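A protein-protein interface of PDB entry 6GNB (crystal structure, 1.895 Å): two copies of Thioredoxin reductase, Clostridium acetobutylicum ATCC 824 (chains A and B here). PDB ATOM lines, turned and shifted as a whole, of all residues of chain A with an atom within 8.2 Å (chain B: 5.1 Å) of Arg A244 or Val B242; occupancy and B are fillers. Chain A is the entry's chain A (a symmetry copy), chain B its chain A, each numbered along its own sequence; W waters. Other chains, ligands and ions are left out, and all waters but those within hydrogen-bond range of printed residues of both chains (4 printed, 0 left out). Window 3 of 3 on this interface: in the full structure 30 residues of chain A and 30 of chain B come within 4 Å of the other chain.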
ATOM      1  N   LYS A 241      -7.903 -11.427  38.110  1.00  0.00           N
ATOM      2  CA  LYS A 241      -8.831 -10.539  37.432  1.00  0.00           C
ATOM      3  C   LYS A 241      -8.165  -9.202  37.127  1.00  0.00           C
ATOM      4  O   LYS A 241      -7.600  -8.559  38.017  1.00  0.00           O
ATOM      5  CB  LYS A 241     -10.074 -10.364  38.286  1.00  0.00           C
ATOM      6  CG  LYS A 241     -10.900 -11.641  38.360  1.00  0.00           C
ATOM      7  CD  LYS A 241     -11.597 -11.905  37.033  1.00  0.00           C
ATOM      8  CE  LYS A 241     -12.410 -13.187  37.061  1.00  0.00           C
ATOM      9  NZ  LYS A 241     -13.064 -13.492  35.758  1.00  0.00           N
ATOM     10  N   VAL A 242      -8.196  -8.812  35.851  1.00  0.00           N
ATOM     11  CA  VAL A 242      -7.596  -7.567  35.395  1.00  0.00           C
ATOM     12  C   VAL A 242      -8.605  -6.773  34.578  1.00  0.00           C
ATOM     13  O   VAL A 242      -9.580  -7.309  34.039  1.00  0.00           O
ATOM     14  CB  VAL A 242      -6.308  -7.764  34.567  1.00  0.00           C
ATOM     15  CG1 VAL A 242      -5.225  -8.462  35.387  1.00  0.00           C
ATOM     16  CG2 VAL A 242      -6.579  -8.550  33.279  1.00  0.00           C
ATOM     17  N   ASN A 243      -8.349  -5.473  34.501  1.00  0.00           N
ATOM     18  CA  ASN A 243      -9.115  -4.591  33.636  1.00  0.00           C
ATOM     19  C   ASN A 243      -8.399  -4.413  32.294  1.00  0.00           C
ATOM     20  O   ASN A 243      -7.430  -5.108  31.965  1.00  0.00           O
ATOM     21  CB  ASN A 243      -9.397  -3.283  34.374  1.00  0.00           C
ATOM     22  CG  ASN A 243      -8.151  -2.447  34.605  1.00  0.00           C
ATOM     23  OD1 ASN A 243      -7.076  -2.709  34.055  1.00  0.00           O
ATOM     24  ND2 ASN A 243      -8.294  -1.421  35.422  1.00  0.00           N
ATOM     25  N   ARG A 244      -8.889  -3.464  31.495  1.00  0.00           N
ATOM     26  CA  ARG A 244      -8.381  -3.263  30.154  1.00  0.00           C
ATOM     27  C   ARG A 244      -6.933  -2.787  30.149  1.00  0.00           C
ATOM     28  O   ARG A 244      -6.265  -2.896  29.117  1.00  0.00           O
ATOM     29  CB  ARG A 244      -9.281  -2.274  29.399  1.00  0.00           C
ATOM     30  CG  ARG A 244     -10.620  -2.870  28.964  1.00  0.00           C
ATOM     31  CD  ARG A 244     -10.496  -3.542  27.608  1.00  0.00           C
ATOM     32  NE  ARG A 244     -10.144  -2.577  26.566  1.00  0.00           N
ATOM     33  CZ  ARG A 244      -9.570  -2.909  25.410  1.00  0.00           C
ATOM     34  NH1 ARG A 244      -9.291  -4.178  25.145  1.00  0.00           N
ATOM     35  NH2 ARG A 244      -9.265  -1.970  24.531  1.00  0.00           N
ATOM     36  N   LYS A 245      -6.448  -2.239  31.260  1.00  0.00           N
ATOM     37  CA  LYS A 245      -5.070  -1.804  31.388  1.00  0.00           C
ATOM     38  C   LYS A 245      -4.184  -2.881  31.995  1.00  0.00           C
ATOM     39  O   LYS A 245      -3.008  -2.611  32.271  1.00  0.00           O
ATOM     40  CB  LYS A 245      -4.995  -0.523  32.216  1.00  0.00           C
ATOM     41  CG  LYS A 245      -5.618   0.676  31.522  1.00  0.00           C
ATOM     42  CD  LYS A 245      -5.510   1.914  32.390  1.00  0.00           C
ATOM     43  CE  LYS A 245      -6.124   3.127  31.722  1.00  0.00           C
ATOM     44  NZ  LYS A 245      -5.082   3.969  31.081  1.00  0.00           N
ATOM     45  N   MET A 246      -4.728  -4.087  32.208  1.00  0.00           N
ATOM     46  CA  MET A 246      -4.030  -5.201  32.844  1.00  0.00           C
ATOM     47  C   MET A 246      -3.766  -4.947  34.316  1.00  0.00           C
ATOM     48  O   MET A 246      -2.948  -5.634  34.924  1.00  0.00           O
ATOM     49  CB  MET A 246      -2.717  -5.574  32.139  1.00  0.00           C
ATOM     50  CG  MET A 246      -2.868  -5.886  30.682  1.00  0.00           C
ATOM     51  SD  MET A 246      -4.053  -7.178  30.308  1.00  0.00           S
ATOM     52  CE  MET A 246      -4.754  -6.512  28.760  1.00  0.00           C
ATOM     53  N   GLU A 247      -4.454  -3.975  34.902  1.00  0.00           N
ATOM     54  CA  GLU A 247      -4.327  -3.677  36.321  1.00  0.00           C
ATOM     55  C   GLU A 247      -5.085  -4.706  37.154  1.00  0.00           C
ATOM     56  O   GLU A 247      -6.238  -5.029  36.857  1.00  0.00           O
ATOM     57  CB  GLU A 247      -4.912  -2.291  36.596  1.00  0.00           C
ATOM     58  CG  GLU A 247      -4.107  -1.168  35.974  1.00  0.00           C
ATOM     59  CD  GLU A 247      -4.820   0.176  35.969  1.00  0.00           C
ATOM     60  OE1 GLU A 247      -6.057   0.220  36.149  1.00  0.00           O
ATOM     61  OE2 GLU A 247      -4.124   1.193  35.774  1.00  0.00           O
ATOM     62  N   TYR A 254       0.224  -5.473  37.917  1.00  0.00           N
ATOM     63  CA  TYR A 254      -0.446  -5.852  36.684  1.00  0.00           C
ATOM     64  C   TYR A 254      -0.352  -7.361  36.516  1.00  0.00           C
ATOM     65  O   TYR A 254       0.436  -8.032  37.194  1.00  0.00           O
ATOM     66  CB  TYR A 254       0.251  -5.177  35.497  1.00  0.00           C
ATOM     67  CG  TYR A 254       0.288  -3.670  35.599  1.00  0.00           C
ATOM     68  CD1 TYR A 254       1.225  -3.036  36.394  1.00  0.00           C
ATOM     69  CD2 TYR A 254      -0.609  -2.889  34.895  1.00  0.00           C
ATOM     70  CE1 TYR A 254       1.261  -1.663  36.501  1.00  0.00           C
ATOM     71  CE2 TYR A 254      -0.580  -1.515  34.992  1.00  0.00           C
ATOM     72  CZ  TYR A 254       0.359  -0.905  35.799  1.00  0.00           C
ATOM     73  OH  TYR A 254       0.408   0.473  35.938  1.00  0.00           O
ATOM     74  N   GLY A 271       0.060  -9.773  23.757  1.00  0.00           N
ATOM     75  CA  GLY A 271      -0.683  -8.518  23.797  1.00  0.00           C
ATOM     76  C   GLY A 271      -0.877  -7.994  25.209  1.00  0.00           C
ATOM     77  O   GLY A 271      -0.688  -6.808  25.483  1.00  0.00           O
ATOM     78  N   GLU A 272      -1.289  -8.871  26.110  1.00  0.00           N
ATOM     79  CA  GLU A 272      -1.436  -8.489  27.516  1.00  0.00           C
ATOM     80  C   GLU A 272      -0.107  -8.056  28.133  1.00  0.00           C
ATOM     81  O   GLU A 272      -0.051  -7.080  28.893  1.00  0.00           O
ATOM     82  CB  GLU A 272      -2.044  -9.654  28.300  1.00  0.00           C
ATOM     83  CG  GLU A 272      -3.504  -9.879  27.940  1.00  0.00           C
ATOM     84  CD  GLU A 272      -4.210 -10.908  28.790  1.00  0.00           C
ATOM     85  OE1 GLU A 272      -3.589 -11.596  29.626  1.00  0.00           O
ATOM     86  OE2 GLU A 272      -5.444 -11.023  28.638  1.00  0.00           O
ATOM     87  N   VAL A 275       0.565  -4.490  26.948  1.00  0.00           N
ATOM     88  CA  VAL A 275      -0.303  -3.498  27.582  1.00  0.00           C
ATOM     89  C   VAL A 275       0.121  -3.250  29.025  1.00  0.00           C
ATOM     90  O   VAL A 275       0.205  -2.100  29.475  1.00  0.00           O
ATOM     91  CB  VAL A 275      -1.771  -3.940  27.485  1.00  0.00           C
ATOM     92  CG1 VAL A 275      -2.660  -2.980  28.286  1.00  0.00           C
ATOM     93  CG2 VAL A 275      -2.217  -3.979  26.031  1.00  0.00           C
ATOM     94  N   ALA A 276       0.414  -4.320  29.756  1.00  0.00           N
ATOM     95  CA  ALA A 276       0.833  -4.165  31.143  1.00  0.00           C
ATOM     96  C   ALA A 276       2.100  -3.327  31.245  1.00  0.00           C
ATOM     97  O   ALA A 276       2.194  -2.426  32.087  1.00  0.00           O
ATOM     98  CB  ALA A 276       1.063  -5.542  31.764  1.00  0.00           C
ATOM     99  N   ASN A 279       1.649   0.429  30.321  1.00  0.00           N
ATOM    100  CA  ASN A 279       0.929   1.128  31.378  1.00  0.00           C
ATOM    101  C   ASN A 279       1.816   1.313  32.599  1.00  0.00           C
ATOM    102  O   ASN A 279       1.845   2.396  33.191  1.00  0.00           O
ATOM    103  CB  ASN A 279      -0.362   0.384  31.720  1.00  0.00           C
ATOM    104  CG  ASN A 279      -1.525   0.817  30.856  1.00  0.00           C
ATOM    105  OD1 ASN A 279      -1.861   1.999  30.816  1.00  0.00           O
ATOM    106  ND2 ASN A 279      -2.135  -0.120  30.146  1.00  0.00           N
ATOM    107  N   ILE B 240     -13.941   2.330  20.589  1.00  0.00           N
ATOM    108  CA  ILE B 240     -14.991   1.343  20.827  1.00  0.00           C
ATOM    109  C   ILE B 240     -14.716   0.654  22.153  1.00  0.00           C
ATOM    110  O   ILE B 240     -13.634   0.100  22.369  1.00  0.00           O
ATOM    111  CB  ILE B 240     -15.055   0.317  19.685  1.00  0.00           C
ATOM    112  CG1 ILE B 240     -15.278   0.998  18.324  1.00  0.00           C
ATOM    113  CG2 ILE B 240     -16.133  -0.723  19.978  1.00  0.00           C
ATOM    114  CD1 ILE B 240     -15.128   0.059  17.122  1.00  0.00           C
ATOM    115  N   LYS B 241     -15.697   0.670  23.047  1.00  0.00           N
ATOM    116  CA  LYS B 241     -15.517   0.109  24.375  1.00  0.00           C
ATOM    117  C   LYS B 241     -15.827  -1.383  24.371  1.00  0.00           C
ATOM    118  O   LYS B 241     -16.896  -1.806  23.919  1.00  0.00           O
ATOM    119  CB  LYS B 241     -16.391   0.862  25.361  1.00  0.00           C
ATOM    120  CG  LYS B 241     -15.905   2.287  25.582  1.00  0.00           C
ATOM    121  CD  LYS B 241     -14.620   2.294  26.399  1.00  0.00           C
ATOM    122  CE  LYS B 241     -14.090   3.700  26.616  1.00  0.00           C
ATOM    123  NZ  LYS B 241     -12.807   3.730  27.373  1.00  0.00           N
ATOM    124  N   VAL B 242     -14.865  -2.181  24.837  1.00  0.00           N
ATOM    125  CA  VAL B 242     -15.002  -3.629  24.891  1.00  0.00           C
ATOM    126  C   VAL B 242     -14.657  -4.132  26.284  1.00  0.00           C
ATOM    127  O   VAL B 242     -13.961  -3.474  27.066  1.00  0.00           O
ATOM    128  CB  VAL B 242     -14.139  -4.375  23.849  1.00  0.00           C
ATOM    129  CG1 VAL B 242     -14.528  -3.981  22.426  1.00  0.00           C
ATOM    130  CG2 VAL B 242     -12.643  -4.125  24.072  1.00  0.00           C
ATOM    131  N   ASN B 243     -15.166  -5.321  26.582  1.00  0.00           N
ATOM    132  CA  ASN B 243     -14.812  -6.023  27.804  1.00  0.00           C
ATOM    133  C   ASN B 243     -13.674  -7.013  27.535  1.00  0.00           C
ATOM    134  O   ASN B 243     -13.041  -7.020  26.473  1.00  0.00           O
ATOM    135  CB  ASN B 243     -16.066  -6.658  28.403  1.00  0.00           C
ATOM    136  CG  ASN B 243     -16.615  -7.799  27.565  1.00  0.00           C
ATOM    137  OD1 ASN B 243     -15.977  -8.288  26.626  1.00  0.00           O
ATOM    138  ND2 ASN B 243     -17.810  -8.240  27.911  1.00  0.00           N
ATOM    139  N   ARG B 244     -13.401  -7.867  28.523  1.00  0.00           N
ATOM    140  CA  ARG B 244     -12.281  -8.782  28.449  1.00  0.00           C
ATOM    141  C   ARG B 244     -12.452  -9.817  27.344  1.00  0.00           C
ATOM    142  O   ARG B 244     -11.463 -10.434  26.936  1.00  0.00           O
ATOM    143  CB  ARG B 244     -12.076  -9.466  29.808  1.00  0.00           C
ATOM    144  CG  ARG B 244     -11.456  -8.555  30.868  1.00  0.00           C
ATOM    145  CD  ARG B 244      -9.939  -8.602  30.799  1.00  0.00           C
ATOM    146  NE  ARG B 244      -9.435  -9.943  31.095  1.00  0.00           N
ATOM    147  CZ  ARG B 244      -8.238 -10.386  30.711  1.00  0.00           C
ATOM    148  NH1 ARG B 244      -7.423  -9.596  30.026  1.00  0.00           N
ATOM    149  NH2 ARG B 244      -7.867 -11.621  31.004  1.00  0.00           N
ATOM    150  N   MET B 246     -13.645  -8.960  24.405  1.00  0.00           N
ATOM    151  CA  MET B 246     -13.693  -8.132  23.204  1.00  0.00           C
ATOM    152  C   MET B 246     -15.114  -7.878  22.738  1.00  0.00           C
ATOM    153  O   MET B 246     -15.325  -7.457  21.603  1.00  0.00           O
ATOM    154  CB  MET B 246     -12.860  -8.698  22.044  1.00  0.00           C
ATOM    155  CG  MET B 246     -11.424  -8.950  22.384  1.00  0.00           C
ATOM    156  SD  MET B 246     -10.541  -7.525  23.020  1.00  0.00           S
ATOM    157  CE  MET B 246      -9.477  -8.350  24.253  1.00  0.00           C
ATOM    158  N   GLU B 247     -16.093  -8.120  23.601  1.00  0.00           N
ATOM    159  CA  GLU B 247     -17.490  -7.861  23.286  1.00  0.00           C
ATOM    160  C   GLU B 247     -17.791  -6.368  23.374  1.00  0.00           C
ATOM    161  O   GLU B 247     -17.412  -5.706  24.343  1.00  0.00           O
ATOM    162  CB  GLU B 247     -18.375  -8.604  24.288  1.00  0.00           C
ATOM    163  CG  GLU B 247     -18.304 -10.110  24.149  1.00  0.00           C
ATOM    164  CD  GLU B 247     -18.923 -10.870  25.312  1.00  0.00           C
ATOM    165  OE1 GLU B 247     -19.136 -10.279  26.393  1.00  0.00           O
ATOM    166  OE2 GLU B 247     -19.188 -12.076  25.132  1.00  0.00           O
ATOM    167  N   THR B 248     -18.490  -5.840  22.376  1.00  0.00           N
ATOM    168  CA  THR B 248     -19.020  -4.485  22.449  1.00  0.00           C
ATOM    169  C   THR B 248     -20.376  -4.522  23.147  1.00  0.00           C
ATOM    170  O   THR B 248     -20.805  -5.565  23.648  1.00  0.00           O
ATOM    171  CB  THR B 248     -19.204  -3.906  21.044  1.00  0.00           C
ATOM    172  OG1 THR B 248     -20.337  -4.529  20.417  1.00  0.00           O
ATOM    173  CG2 THR B 248     -17.947  -4.079  20.170  1.00  0.00           C
ATOM    174  N   ALA B 255     -14.828  -6.214  18.938  1.00  0.00           N
ATOM    175  CA  ALA B 255     -13.903  -5.244  18.360  1.00  0.00           C
ATOM    176  C   ALA B 255     -12.495  -5.567  18.841  1.00  0.00           C
ATOM    177  O   ALA B 255     -12.309  -6.084  19.945  1.00  0.00           O
ATOM    178  CB  ALA B 255     -14.295  -3.814  18.735  1.00  0.00           C
ATOM    179  N   THR B 260     -10.176  -0.236  19.477  1.00  0.00           N
ATOM    180  CA  THR B 260     -10.600  -0.352  20.873  1.00  0.00           C
ATOM    181  C   THR B 260      -9.908   0.591  21.899  1.00  0.00           C
ATOM    182  O   THR B 260     -10.266   0.539  23.074  1.00  0.00           O
ATOM    183  CB  THR B 260     -10.444  -1.796  21.389  1.00  0.00           C
ATOM    184  OG1 THR B 260      -9.058  -2.089  21.602  1.00  0.00           O
ATOM    185  CG2 THR B 260     -11.034  -2.787  20.400  1.00  0.00           C
ATOM    186  N   GLY B 261      -8.953   1.447  21.510  1.00  0.00           N
ATOM    187  CA  GLY B 261      -8.299   2.311  22.469  1.00  0.00           C
ATOM    188  C   GLY B 261      -6.801   2.091  22.492  1.00  0.00           C
ATOM    189  O   GLY B 261      -6.274   1.194  21.833  1.00  0.00           O
ATOM    190  N   LYS B 268      -0.764  -5.895  21.061  1.00  0.00           N
ATOM    191  CA  LYS B 268      -2.101  -5.679  21.601  1.00  0.00           C
ATOM    192  C   LYS B 268      -3.150  -6.019  20.550  1.00  0.00           C
ATOM    193  O   LYS B 268      -4.108  -6.750  20.818  1.00  0.00           O
ATOM    194  CB  LYS B 268      -2.269  -4.235  22.067  1.00  0.00           C
ATOM    195  CG  LYS B 268      -3.715  -3.945  22.522  1.00  0.00           C
ATOM    196  CD  LYS B 268      -3.995  -2.522  22.980  1.00  0.00           C
ATOM    197  CE  LYS B 268      -4.650  -1.633  21.902  1.00  0.00           C
ATOM    198  NZ  LYS B 268      -6.043  -1.918  21.413  1.00  0.00           N
ATOM    199  N   GLU B 272      -5.956  -9.051  20.831  1.00  0.00           N
ATOM    200  CA  GLU B 272      -7.387  -8.742  20.796  1.00  0.00           C
ATOM    201  C   GLU B 272      -8.098  -9.446  19.642  1.00  0.00           C
ATOM    202  O   GLU B 272      -9.214  -9.958  19.802  1.00  0.00           O
ATOM    203  CB  GLU B 272      -7.580  -7.226  20.708  1.00  0.00           C
ATOM    204  CG  GLU B 272      -7.197  -6.530  22.004  1.00  0.00           C
ATOM    205  CD  GLU B 272      -7.511  -5.054  22.041  1.00  0.00           C
ATOM    206  OE1 GLU B 272      -7.931  -4.454  21.031  1.00  0.00           O
ATOM    207  OE2 GLU B 272      -7.357  -4.465  23.132  1.00  0.00           O
HETATM  208  O   HOH W   1      -8.723 -11.160  34.082  1.00  0.00           O
HETATM  209  O   HOH W   2     -12.243  -0.751  24.785  1.00  0.00           O
HETATM  210  O   HOH W   3     -10.412  -6.281  26.646  1.00  0.00           O
HETATM  211  O   HOH W   4      -7.847  -6.816  29.867  1.00  0.00           O
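Val A242 touches Arg B244, and with the chains exchanged Arg A244 touches Val B242. Arg A244 touches Glu B272, and with the chains exchanged Glu A272 touches Arg B244. Of the 7 pairs that touch across the chains among the printed residues, 4 have their exchanged pair printed and touching as well.
O of Val A275 lies within hydrogen-bond range of ND2 of Asn A279, at 3.1 Å. The side-chain amino group of Lys B268 lies within salt-bridge range of the side-chain carboxylate of Glu B272, 3.2 Å away. The side-chain amino group (NZ) of Lys B268 lies within hydrogen-bond range of the backbone carbonyl oxygen (O) of Gly B261, at 3.1 Å. OG1 of Thr B260 is in hydrogen-bond range of OE1 of Glu B272 (2.7 Å). NZ of Lys B268 is in hydrogen-bond range of OG1 of Thr B260 (3.0 Å).
Arg B244 touches Val A242 (CD to O, 3.5 Å). CD of Arg A244 touches O of Val B242 (3.5 Å). Gly A271 touches Lys B268. Lys B268 touches Val A275 (CG to CG2, 3.8 Å).
The side-chain carboxylate of Glu B272 is in salt-bridge range of the guanidinium group of Arg A244. The side-chain carboxylate of Glu A272 lies within salt-bridge range of the guanidinium group of Arg B244 (2.8 Å). The side-chain hydroxyl of Thr B260 lies within hydrogen-bond range of the guanidinium group of Arg A244 (2.9 Å).
Printed residues of chain B within 4 Å of Arg A244: Val B242, Thr B260 and Glu B272. Val B242 touches just one residue of chain A: Arg A244. Of the printed residues of chain B, Val A275 touches Lys B268. Printed residues of chain A within 4 Å of Thr B260: Arg A244 (2.9 Å). Glu A247 touches none of the printed residues of chain B. The nearest printed residue of chain B that does not touch Arg A244 is Met B246 (4.2 Å). The nearest residue of chain A that does not touch Val B242 is Asn A243 (7.7 Å). The nearest printed residue of chain A that does not touch Arg B244 is Met A246 (4.2 Å).
Water W3 bridges the backbone carbonyl oxygen (O) of Asn B243 (2.7 Å) and the guanidinium group (NH1) of Arg A244 (2.8 Å). Water W4 lies within hydrogen-bond range of O of Asn A243 and NH1 of Arg B244. Water W2 lies within hydrogen-bond range of the backbone carbonyl oxygen (O) of Ile B240 (2.9 Å), the backbone carbonyl oxygen (O) of Thr B260 (2.9 Å), the backbone NH (N) of Val B242 (3.0 Å) and the guanidinium group (NH2) of Arg A244 (3.2 Å). Water W1 bridges the backbone NH (N) of Val A242 (3.0 Å) and the guanidinium group (NH2) of Arg B244 (3.2 Å).
Of the 13 printed residues of chain A, 5 touch a printed residue of chain B. Hydrophobic or aromatic side chains of chain A within 4 Å of the printed part of chain B: Val A242 and Val A275. Hydrophobic or aromatic side chains of chain B within 4 Å of the printed part of chain A: Val B242. Among the printed residues, 7 pairs touch across the chains. Among the printed residues, Asp or Glu carboxylates within 4 Å of a Lys or Arg side-chain nitrogen of the other chain: Arg A244 with Glu B272 (2.8 Å) and Glu A272 with Arg B244 (2.8 Å).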
